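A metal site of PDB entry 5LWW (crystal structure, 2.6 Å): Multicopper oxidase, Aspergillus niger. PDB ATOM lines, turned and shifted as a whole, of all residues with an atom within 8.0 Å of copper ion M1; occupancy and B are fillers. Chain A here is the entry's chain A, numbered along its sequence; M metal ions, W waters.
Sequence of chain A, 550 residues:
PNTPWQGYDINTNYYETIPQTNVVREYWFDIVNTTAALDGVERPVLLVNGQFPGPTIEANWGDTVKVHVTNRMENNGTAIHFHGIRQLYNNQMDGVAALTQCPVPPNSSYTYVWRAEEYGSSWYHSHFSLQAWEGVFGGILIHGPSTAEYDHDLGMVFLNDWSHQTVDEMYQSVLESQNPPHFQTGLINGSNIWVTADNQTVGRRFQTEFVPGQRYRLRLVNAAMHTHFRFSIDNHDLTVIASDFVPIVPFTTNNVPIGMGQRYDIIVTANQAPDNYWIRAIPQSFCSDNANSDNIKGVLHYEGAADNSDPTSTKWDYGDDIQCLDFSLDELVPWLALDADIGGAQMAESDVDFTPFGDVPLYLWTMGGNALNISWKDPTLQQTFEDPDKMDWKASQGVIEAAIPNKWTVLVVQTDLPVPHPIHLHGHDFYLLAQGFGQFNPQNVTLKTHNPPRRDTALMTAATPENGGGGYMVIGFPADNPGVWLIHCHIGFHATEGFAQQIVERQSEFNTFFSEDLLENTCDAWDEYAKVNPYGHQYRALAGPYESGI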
ATOM      1  N   HIS A  81      -8.022 -11.139   6.253  1.00  0.00           N
ATOM      2  CA  HIS A  81      -9.127 -10.195   6.146  1.00  0.00           C
ATOM      3  C   HIS A  81      -9.950 -10.575   4.905  1.00  0.00           C
ATOM      4  O   HIS A  81      -9.398 -10.981   3.864  1.00  0.00           O
ATOM      5  CB  HIS A  81      -8.565  -8.771   6.069  1.00  0.00           C
ATOM      6  CG  HIS A  81      -9.600  -7.727   5.771  1.00  0.00           C
ATOM      7  ND1 HIS A  81     -10.642  -7.443   6.633  1.00  0.00           N
ATOM      8  CD2 HIS A  81      -9.767  -6.911   4.708  1.00  0.00           C
ATOM      9  CE1 HIS A  81     -11.399  -6.500   6.122  1.00  0.00           C
ATOM     10  NE2 HIS A  81     -10.896  -6.159   4.952  1.00  0.00           N
ATOM     11  N   PHE A  82     -11.255 -10.494   5.034  1.00  0.00           N
ATOM     12  CA  PHE A  82     -12.146 -10.774   3.950  1.00  0.00           C
ATOM     13  C   PHE A  82     -12.611  -9.386   3.502  1.00  0.00           C
ATOM     14  O   PHE A  82     -13.513  -8.783   4.094  1.00  0.00           O
ATOM     15  CB  PHE A  82     -13.240 -11.752   4.444  1.00  0.00           C
ATOM     16  CG  PHE A  82     -12.652 -12.992   5.067  1.00  0.00           C
ATOM     17  CD1 PHE A  82     -12.270 -12.995   6.419  1.00  0.00           C
ATOM     18  CD2 PHE A  82     -12.367 -14.124   4.293  1.00  0.00           C
ATOM     19  CE1 PHE A  82     -11.643 -14.104   6.970  1.00  0.00           C
ATOM     20  CE2 PHE A  82     -11.737 -15.243   4.843  1.00  0.00           C
ATOM     21  CZ  PHE A  82     -11.376 -15.228   6.182  1.00  0.00           C
ATOM     22  N   HIS A  83     -11.957  -8.877   2.477  1.00  0.00           N
ATOM     23  CA  HIS A  83     -12.190  -7.521   2.016  1.00  0.00           C
ATOM     24  C   HIS A  83     -13.666  -7.290   1.554  1.00  0.00           C
ATOM     25  O   HIS A  83     -14.239  -8.065   0.768  1.00  0.00           O
ATOM     26  CB  HIS A  83     -11.121  -7.176   0.938  1.00  0.00           C
ATOM     27  CG  HIS A  83     -11.158  -5.766   0.452  1.00  0.00           C
ATOM     28  ND1 HIS A  83     -10.080  -4.897   0.577  1.00  0.00           N
ATOM     29  CD2 HIS A  83     -12.120  -5.056  -0.187  1.00  0.00           C
ATOM     30  CE1 HIS A  83     -10.385  -3.734   0.050  1.00  0.00           C
ATOM     31  NE2 HIS A  83     -11.622  -3.793  -0.407  1.00  0.00           N
ATOM     32  N   GLY A  84     -14.310  -6.231   2.061  1.00  0.00           N
ATOM     33  CA  GLY A  84     -15.664  -5.904   1.612  1.00  0.00           C
ATOM     34  C   GLY A  84     -16.771  -6.668   2.344  1.00  0.00           C
ATOM     35  O   GLY A  84     -17.955  -6.316   2.238  1.00  0.00           O
ATOM     36  N   SER A 122     -15.116 -10.163  -4.442  1.00  0.00           N
ATOM     37  CA  SER A 122     -14.086  -9.518  -3.659  1.00  0.00           C
ATOM     38  C   SER A 122     -12.918 -10.501  -3.556  1.00  0.00           C
ATOM     39  O   SER A 122     -12.679 -11.315  -4.479  1.00  0.00           O
ATOM     40  CB  SER A 122     -14.635  -9.123  -2.279  1.00  0.00           C
ATOM     41  OG  SER A 122     -13.886  -8.106  -1.654  1.00  0.00           O
ATOM     42  N   TRP A 123     -12.200 -10.395  -2.438  1.00  0.00           N
ATOM     43  CA  TRP A 123     -10.993 -11.173  -2.169  1.00  0.00           C
ATOM     44  C   TRP A 123     -10.675 -11.115  -0.673  1.00  0.00           C
ATOM     45  O   TRP A 123     -11.137 -10.219   0.048  1.00  0.00           O
ATOM     46  CB  TRP A 123      -9.812 -10.657  -3.024  1.00  0.00           C
ATOM     47  CG  TRP A 123      -9.437  -9.163  -2.901  1.00  0.00           C
ATOM     48  CD1 TRP A 123     -10.282  -8.064  -2.904  1.00  0.00           C
ATOM     49  CD2 TRP A 123      -8.111  -8.626  -2.839  1.00  0.00           C
ATOM     50  NE1 TRP A 123      -9.563  -6.886  -2.804  1.00  0.00           N
ATOM     51  CE2 TRP A 123      -8.222  -7.205  -2.786  1.00  0.00           C
ATOM     52  CE3 TRP A 123      -6.844  -9.207  -2.817  1.00  0.00           C
ATOM     53  CZ2 TRP A 123      -7.112  -6.364  -2.716  1.00  0.00           C
ATOM     54  CZ3 TRP A 123      -5.733  -8.357  -2.736  1.00  0.00           C
ATOM     55  CH2 TRP A 123      -5.882  -6.954  -2.681  1.00  0.00           C
ATOM     56  N   TYR A 124      -9.917 -12.124  -0.208  1.00  0.00           N
ATOM     57  CA  TYR A 124      -9.354 -12.180   1.129  1.00  0.00           C
ATOM     58  C   TYR A 124      -7.862 -11.968   0.935  1.00  0.00           C
ATOM     59  O   TYR A 124      -7.326 -12.302  -0.129  1.00  0.00           O
ATOM     60  CB  TYR A 124      -9.573 -13.560   1.774  1.00  0.00           C
ATOM     61  CG  TYR A 124      -8.979 -14.732   1.013  1.00  0.00           C
ATOM     62  CD1 TYR A 124      -7.673 -15.109   1.201  1.00  0.00           C
ATOM     63  CD2 TYR A 124      -9.740 -15.436   0.087  1.00  0.00           C
ATOM     64  CE1 TYR A 124      -7.115 -16.183   0.500  1.00  0.00           C
ATOM     65  CE2 TYR A 124      -9.204 -16.501  -0.637  1.00  0.00           C
ATOM     66  CZ  TYR A 124      -7.898 -16.872  -0.417  1.00  0.00           C
ATOM     67  OH  TYR A 124      -7.319 -17.910  -1.124  1.00  0.00           O
ATOM     68  N   HIS A 125      -7.177 -11.441   1.923  1.00  0.00           N
ATOM     69  CA  HIS A 125      -5.737 -11.320   1.797  1.00  0.00           C
ATOM     70  C   HIS A 125      -5.209 -11.049   3.173  1.00  0.00           C
ATOM     71  O   HIS A 125      -6.003 -10.840   4.069  1.00  0.00           O
ATOM     72  CB  HIS A 125      -5.350 -10.185   0.834  1.00  0.00           C
ATOM     73  CG  HIS A 125      -6.001  -8.857   1.143  1.00  0.00           C
ATOM     74  ND1 HIS A 125      -5.679  -8.102   2.254  1.00  0.00           N
ATOM     75  CD2 HIS A 125      -6.903  -8.126   0.441  1.00  0.00           C
ATOM     76  CE1 HIS A 125      -6.375  -6.979   2.229  1.00  0.00           C
ATOM     77  NE2 HIS A 125      -7.131  -6.973   1.142  1.00  0.00           N
ATOM     78  N   SER A 126      -3.899 -11.032   3.345  1.00  0.00           N
ATOM     79  CA  SER A 126      -3.357 -10.771   4.661  1.00  0.00           C
ATOM     80  C   SER A 126      -3.524  -9.329   5.033  1.00  0.00           C
ATOM     81  O   SER A 126      -3.440  -8.426   4.191  1.00  0.00           O
ATOM     82  CB  SER A 126      -1.887 -11.129   4.800  1.00  0.00           C
ATOM     83  OG  SER A 126      -1.708 -12.488   4.523  1.00  0.00           O
ATOM     84  N   HIS A 127      -3.775  -9.127   6.317  1.00  0.00           N
ATOM     85  CA  HIS A 127      -3.684  -7.813   6.834  1.00  0.00           C
ATOM     86  C   HIS A 127      -2.564  -7.920   7.859  1.00  0.00           C
ATOM     87  O   HIS A 127      -2.734  -7.604   9.022  1.00  0.00           O
ATOM     88  CB  HIS A 127      -5.025  -7.415   7.428  1.00  0.00           C
ATOM     89  CG  HIS A 127      -5.478  -6.057   6.995  1.00  0.00           C
ATOM     90  ND1 HIS A 127      -4.827  -4.907   7.374  1.00  0.00           N
ATOM     91  CD2 HIS A 127      -6.502  -5.669   6.193  1.00  0.00           C
ATOM     92  CE1 HIS A 127      -5.444  -3.860   6.838  1.00  0.00           C
ATOM     93  NE2 HIS A 127      -6.478  -4.298   6.130  1.00  0.00           N
ATOM     94  N   ALA A 132       0.097  -9.580   2.175  1.00  0.00           N
ATOM     95  CA  ALA A 132      -0.892  -9.730   1.123  1.00  0.00           C
ATOM     96  C   ALA A 132      -0.186  -9.668  -0.198  1.00  0.00           C
ATOM     97  O   ALA A 132      -0.525 -10.410  -1.099  1.00  0.00           O
ATOM     98  CB  ALA A 132      -1.979  -8.662   1.217  1.00  0.00           C
ATOM     99  N   TRP A 133       0.827  -8.806  -0.294  1.00  0.00           N
ATOM    100  CA  TRP A 133       1.601  -8.605  -1.537  1.00  0.00           C
ATOM    101  C   TRP A 133       2.765  -9.587  -1.784  1.00  0.00           C
ATOM    102  O   TRP A 133       3.435  -9.495  -2.813  1.00  0.00           O
ATOM    103  CB  TRP A 133       1.991  -7.135  -1.698  1.00  0.00           C
ATOM    104  CG  TRP A 133       0.768  -6.340  -1.630  1.00  0.00           C
ATOM    105  CD1 TRP A 133      -0.052  -6.005  -2.658  1.00  0.00           C
ATOM    106  CD2 TRP A 133       0.136  -5.855  -0.449  1.00  0.00           C
ATOM    107  NE1 TRP A 133      -1.141  -5.303  -2.185  1.00  0.00           N
ATOM    108  CE2 TRP A 133      -1.038  -5.200  -0.833  1.00  0.00           C
ATOM    109  CE3 TRP A 133       0.476  -5.908   0.905  1.00  0.00           C
ATOM    110  CZ2 TRP A 133      -1.880  -4.602   0.078  1.00  0.00           C
ATOM    111  CZ3 TRP A 133      -0.386  -5.297   1.834  1.00  0.00           C
ATOM    112  CH2 TRP A 133      -1.545  -4.665   1.413  1.00  0.00           C
ATOM    113  N   ASN A 222      -8.206  -5.407  -8.453  1.00  0.00           N
ATOM    114  CA  ASN A 222      -6.863  -4.849  -8.450  1.00  0.00           C
ATOM    115  C   ASN A 222      -6.151  -5.211  -7.128  1.00  0.00           C
ATOM    116  O   ASN A 222      -6.391  -4.598  -6.074  1.00  0.00           O
ATOM    117  CB  ASN A 222      -6.865  -3.346  -8.710  1.00  0.00           C
ATOM    118  CG  ASN A 222      -5.448  -2.775  -8.765  1.00  0.00           C
ATOM    119  OD1 ASN A 222      -4.460  -3.444  -8.421  1.00  0.00           O
ATOM    120  ND2 ASN A 222      -5.329  -1.524  -9.199  1.00  0.00           N
ATOM    121  N   MET A 260      -6.701   0.109  -6.395  1.00  0.00           N
ATOM    122  CA  MET A 260      -6.254  -1.001  -5.554  1.00  0.00           C
ATOM    123  C   MET A 260      -7.213  -1.374  -4.401  1.00  0.00           C
ATOM    124  O   MET A 260      -7.503  -0.563  -3.533  1.00  0.00           O
ATOM    125  CB  MET A 260      -4.871  -0.725  -5.024  1.00  0.00           C
ATOM    126  CG  MET A 260      -3.815  -0.932  -6.069  1.00  0.00           C
ATOM    127  SD  MET A 260      -2.269  -0.304  -5.444  1.00  0.00           S
ATOM    128  CE  MET A 260      -2.477   1.406  -5.982  1.00  0.00           C
ATOM    129  N   GLY A 261      -7.677  -2.621  -4.416  1.00  0.00           N
ATOM    130  CA  GLY A 261      -8.682  -3.111  -3.475  1.00  0.00           C
ATOM    131  C   GLY A 261     -10.097  -3.082  -4.033  1.00  0.00           C
ATOM    132  O   GLY A 261     -11.006  -3.692  -3.462  1.00  0.00           O
ATOM    133  N   GLN A 262     -10.297  -2.362  -5.131  1.00  0.00           N
ATOM    134  CA  GLN A 262     -11.604  -2.263  -5.736  1.00  0.00           C
ATOM    135  C   GLN A 262     -11.921  -3.530  -6.520  1.00  0.00           C
ATOM    136  O   GLN A 262     -11.032  -4.273  -6.911  1.00  0.00           O
ATOM    137  CB  GLN A 262     -11.626  -1.091  -6.686  1.00  0.00           C
ATOM    138  CG  GLN A 262     -11.583   0.277  -6.021  1.00  0.00           C
ATOM    139  CD  GLN A 262     -11.718   1.384  -7.061  1.00  0.00           C
ATOM    140  OE1 GLN A 262     -11.478   1.147  -8.247  1.00  0.00           O
ATOM    141  NE2 GLN A 262     -12.131   2.583  -6.632  1.00  0.00           N
ATOM    142  N   ARG A 263     -13.206  -3.767  -6.775  1.00  0.00           N
ATOM    143  CA  ARG A 263     -13.612  -4.804  -7.740  1.00  0.00           C
ATOM    144  C   ARG A 263     -14.609  -4.218  -8.692  1.00  0.00           C
ATOM    145  O   ARG A 263     -15.398  -3.337  -8.320  1.00  0.00           O
ATOM    146  CB  ARG A 263     -14.232  -6.016  -7.058  1.00  0.00           C
ATOM    147  CG  ARG A 263     -13.278  -6.763  -6.130  1.00  0.00           C
ATOM    148  CD  ARG A 263     -13.191  -6.077  -4.777  1.00  0.00           C
ATOM    149  NE  ARG A 263     -14.480  -6.041  -4.080  1.00  0.00           N
ATOM    150  CZ  ARG A 263     -14.696  -5.281  -3.007  1.00  0.00           C
ATOM    151  NH1 ARG A 263     -13.708  -4.489  -2.576  1.00  0.00           N
ATOM    152  NH2 ARG A 263     -15.861  -5.304  -2.370  1.00  0.00           N
ATOM    153  N   HIS A 424     -10.103   2.690   1.765  1.00  0.00           N
ATOM    154  CA  HIS A 424     -10.918   1.538   1.967  1.00  0.00           C
ATOM    155  C   HIS A 424     -11.429   1.567   3.381  1.00  0.00           C
ATOM    156  O   HIS A 424     -10.662   1.810   4.305  1.00  0.00           O
ATOM    157  CB  HIS A 424     -10.063   0.303   1.747  1.00  0.00           C
ATOM    158  CG  HIS A 424     -10.733  -0.957   2.158  1.00  0.00           C
ATOM    159  ND1 HIS A 424     -12.061  -1.203   1.897  1.00  0.00           N
ATOM    160  CD2 HIS A 424     -10.265  -2.058   2.789  1.00  0.00           C
ATOM    161  CE1 HIS A 424     -12.383  -2.397   2.354  1.00  0.00           C
ATOM    162  NE2 HIS A 424     -11.307  -2.936   2.884  1.00  0.00           N
ATOM    163  N   HIS A 426     -13.204  -0.635   6.315  1.00  0.00           N
ATOM    164  CA  HIS A 426     -13.600  -1.933   6.827  1.00  0.00           C
ATOM    165  C   HIS A 426     -14.990  -1.794   7.437  1.00  0.00           C
ATOM    166  O   HIS A 426     -15.374  -0.712   7.861  1.00  0.00           O
ATOM    167  CB  HIS A 426     -12.631  -2.397   7.911  1.00  0.00           C
ATOM    168  CG  HIS A 426     -11.307  -2.880   7.394  1.00  0.00           C
ATOM    169  ND1 HIS A 426     -10.793  -4.119   7.715  1.00  0.00           N
ATOM    170  CD2 HIS A 426     -10.393  -2.291   6.576  1.00  0.00           C
ATOM    171  CE1 HIS A 426      -9.614  -4.272   7.117  1.00  0.00           C
ATOM    172  NE2 HIS A 426      -9.362  -3.187   6.414  1.00  0.00           N
ATOM    173  N   ASP A 456     -16.702   0.173  -1.055  1.00  0.00           N
ATOM    174  CA  ASP A 456     -15.835   0.035   0.125  1.00  0.00           C
ATOM    175  C   ASP A 456     -14.436   0.609  -0.072  1.00  0.00           C
ATOM    176  O   ASP A 456     -13.718   0.824   0.911  1.00  0.00           O
ATOM    177  CB  ASP A 456     -15.817  -1.406   0.659  1.00  0.00           C
ATOM    178  CG  ASP A 456     -15.153  -2.366  -0.277  1.00  0.00           C
ATOM    179  OD1 ASP A 456     -14.017  -2.076  -0.711  1.00  0.00           O
ATOM    180  OD2 ASP A 456     -15.748  -3.424  -0.556  1.00  0.00           O
ATOM    181  N   THR A 457     -14.064   0.862  -1.337  1.00  0.00           N
ATOM    182  CA  THR A 457     -12.797   1.470  -1.697  1.00  0.00           C
ATOM    183  C   THR A 457     -12.975   2.515  -2.810  1.00  0.00           C
ATOM    184  O   THR A 457     -13.580   2.248  -3.848  1.00  0.00           O
ATOM    185  CB  THR A 457     -11.868   0.377  -2.193  1.00  0.00           C
ATOM    186  OG1 THR A 457     -11.903  -0.713  -1.250  1.00  0.00           O
ATOM    187  CG2 THR A 457     -10.408   0.920  -2.457  1.00  0.00           C
ATOM    188  N   HIS A 488      -8.130   3.108   5.763  1.00  0.00           N
ATOM    189  CA  HIS A 488      -6.753   3.178   5.359  1.00  0.00           C
ATOM    190  C   HIS A 488      -6.536   3.220   3.875  1.00  0.00           C
ATOM    191  O   HIS A 488      -7.431   2.934   3.081  1.00  0.00           O
ATOM    192  CB  HIS A 488      -5.958   1.986   5.951  1.00  0.00           C
ATOM    193  CG  HIS A 488      -6.217   0.677   5.272  1.00  0.00           C
ATOM    194  ND1 HIS A 488      -5.328   0.094   4.409  1.00  0.00           N
ATOM    195  CD2 HIS A 488      -7.293  -0.149   5.308  1.00  0.00           C
ATOM    196  CE1 HIS A 488      -5.828  -1.044   3.943  1.00  0.00           C
ATOM    197  NE2 HIS A 488      -7.027  -1.215   4.469  1.00  0.00           N
ATOM    198  N   HIS A 490      -5.262   1.648   0.652  1.00  0.00           N
ATOM    199  CA  HIS A 490      -5.121   0.265   0.249  1.00  0.00           C
ATOM    200  C   HIS A 490      -3.789  -0.032  -0.422  1.00  0.00           C
ATOM    201  O   HIS A 490      -3.530  -1.175  -0.814  1.00  0.00           O
ATOM    202  CB  HIS A 490      -6.291  -0.225  -0.603  1.00  0.00           C
ATOM    203  CG  HIS A 490      -6.539  -1.705  -0.453  1.00  0.00           C
ATOM    204  ND1 HIS A 490      -5.767  -2.661  -1.077  1.00  0.00           N
ATOM    205  CD2 HIS A 490      -7.450  -2.377   0.286  1.00  0.00           C
ATOM    206  CE1 HIS A 490      -6.192  -3.862  -0.732  1.00  0.00           C
ATOM    207  NE2 HIS A 490      -7.222  -3.716   0.099  1.00  0.00           N
HETATM  208 CU    CU M   1      -8.247  -5.237   1.107  1.00  0.00          CU
HETATM  209 CU    CU M   2     -11.110  -4.567   3.942  1.00  0.00          CU
HETATM  210 CU    CU M   3      -7.702  -3.243   4.995  1.00  0.00          CU
HETATM  211  O   HOH W   1      -7.878  -4.102   3.145  1.00  0.00           O
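N of His 83 is in hydrogen-bond range of O of Trp 123, at 2.9 Å. The backbone NH (N) of His 125 is in hydrogen-bond range of the backbone carbonyl oxygen (O) of His 81 (3.0 Å). The side-chain hydroxyl of Ser 122 lies within hydrogen-bond range of the backbone carbonyl oxygen of His 83 (2.4 Å). A ring nitrogen (NE2) of His 83 is in hydrogen-bond range of the side-chain carboxylate (OD1) of Asp 456 (3.0 Å). NE2 of His 83 lies within hydrogen-bond range of O of Gly 261, 3.1 Å away. NE2 of His 83 is in hydrogen-bond range of OG1 of Thr 457, 3.2 Å away. A ring nitrogen (NE2) of His 83 lies close to a ring nitrogen (ND1) of His 424, 3.5 Å away. A ring nitrogen (NE2) of His 83 lies close to the guanidinium group (NH1) of Arg 263.
ND1 of His 83 is bound to copper ion M1, 1.9 Å away. Copper ion M1 is bound by a ring nitrogen (NE2) of His 125 (2.1 Å). NE2 of His 490 is bound to copper ion M1, 2.1 Å away. Water W1 binds copper ion M1, at 2.4 Å.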
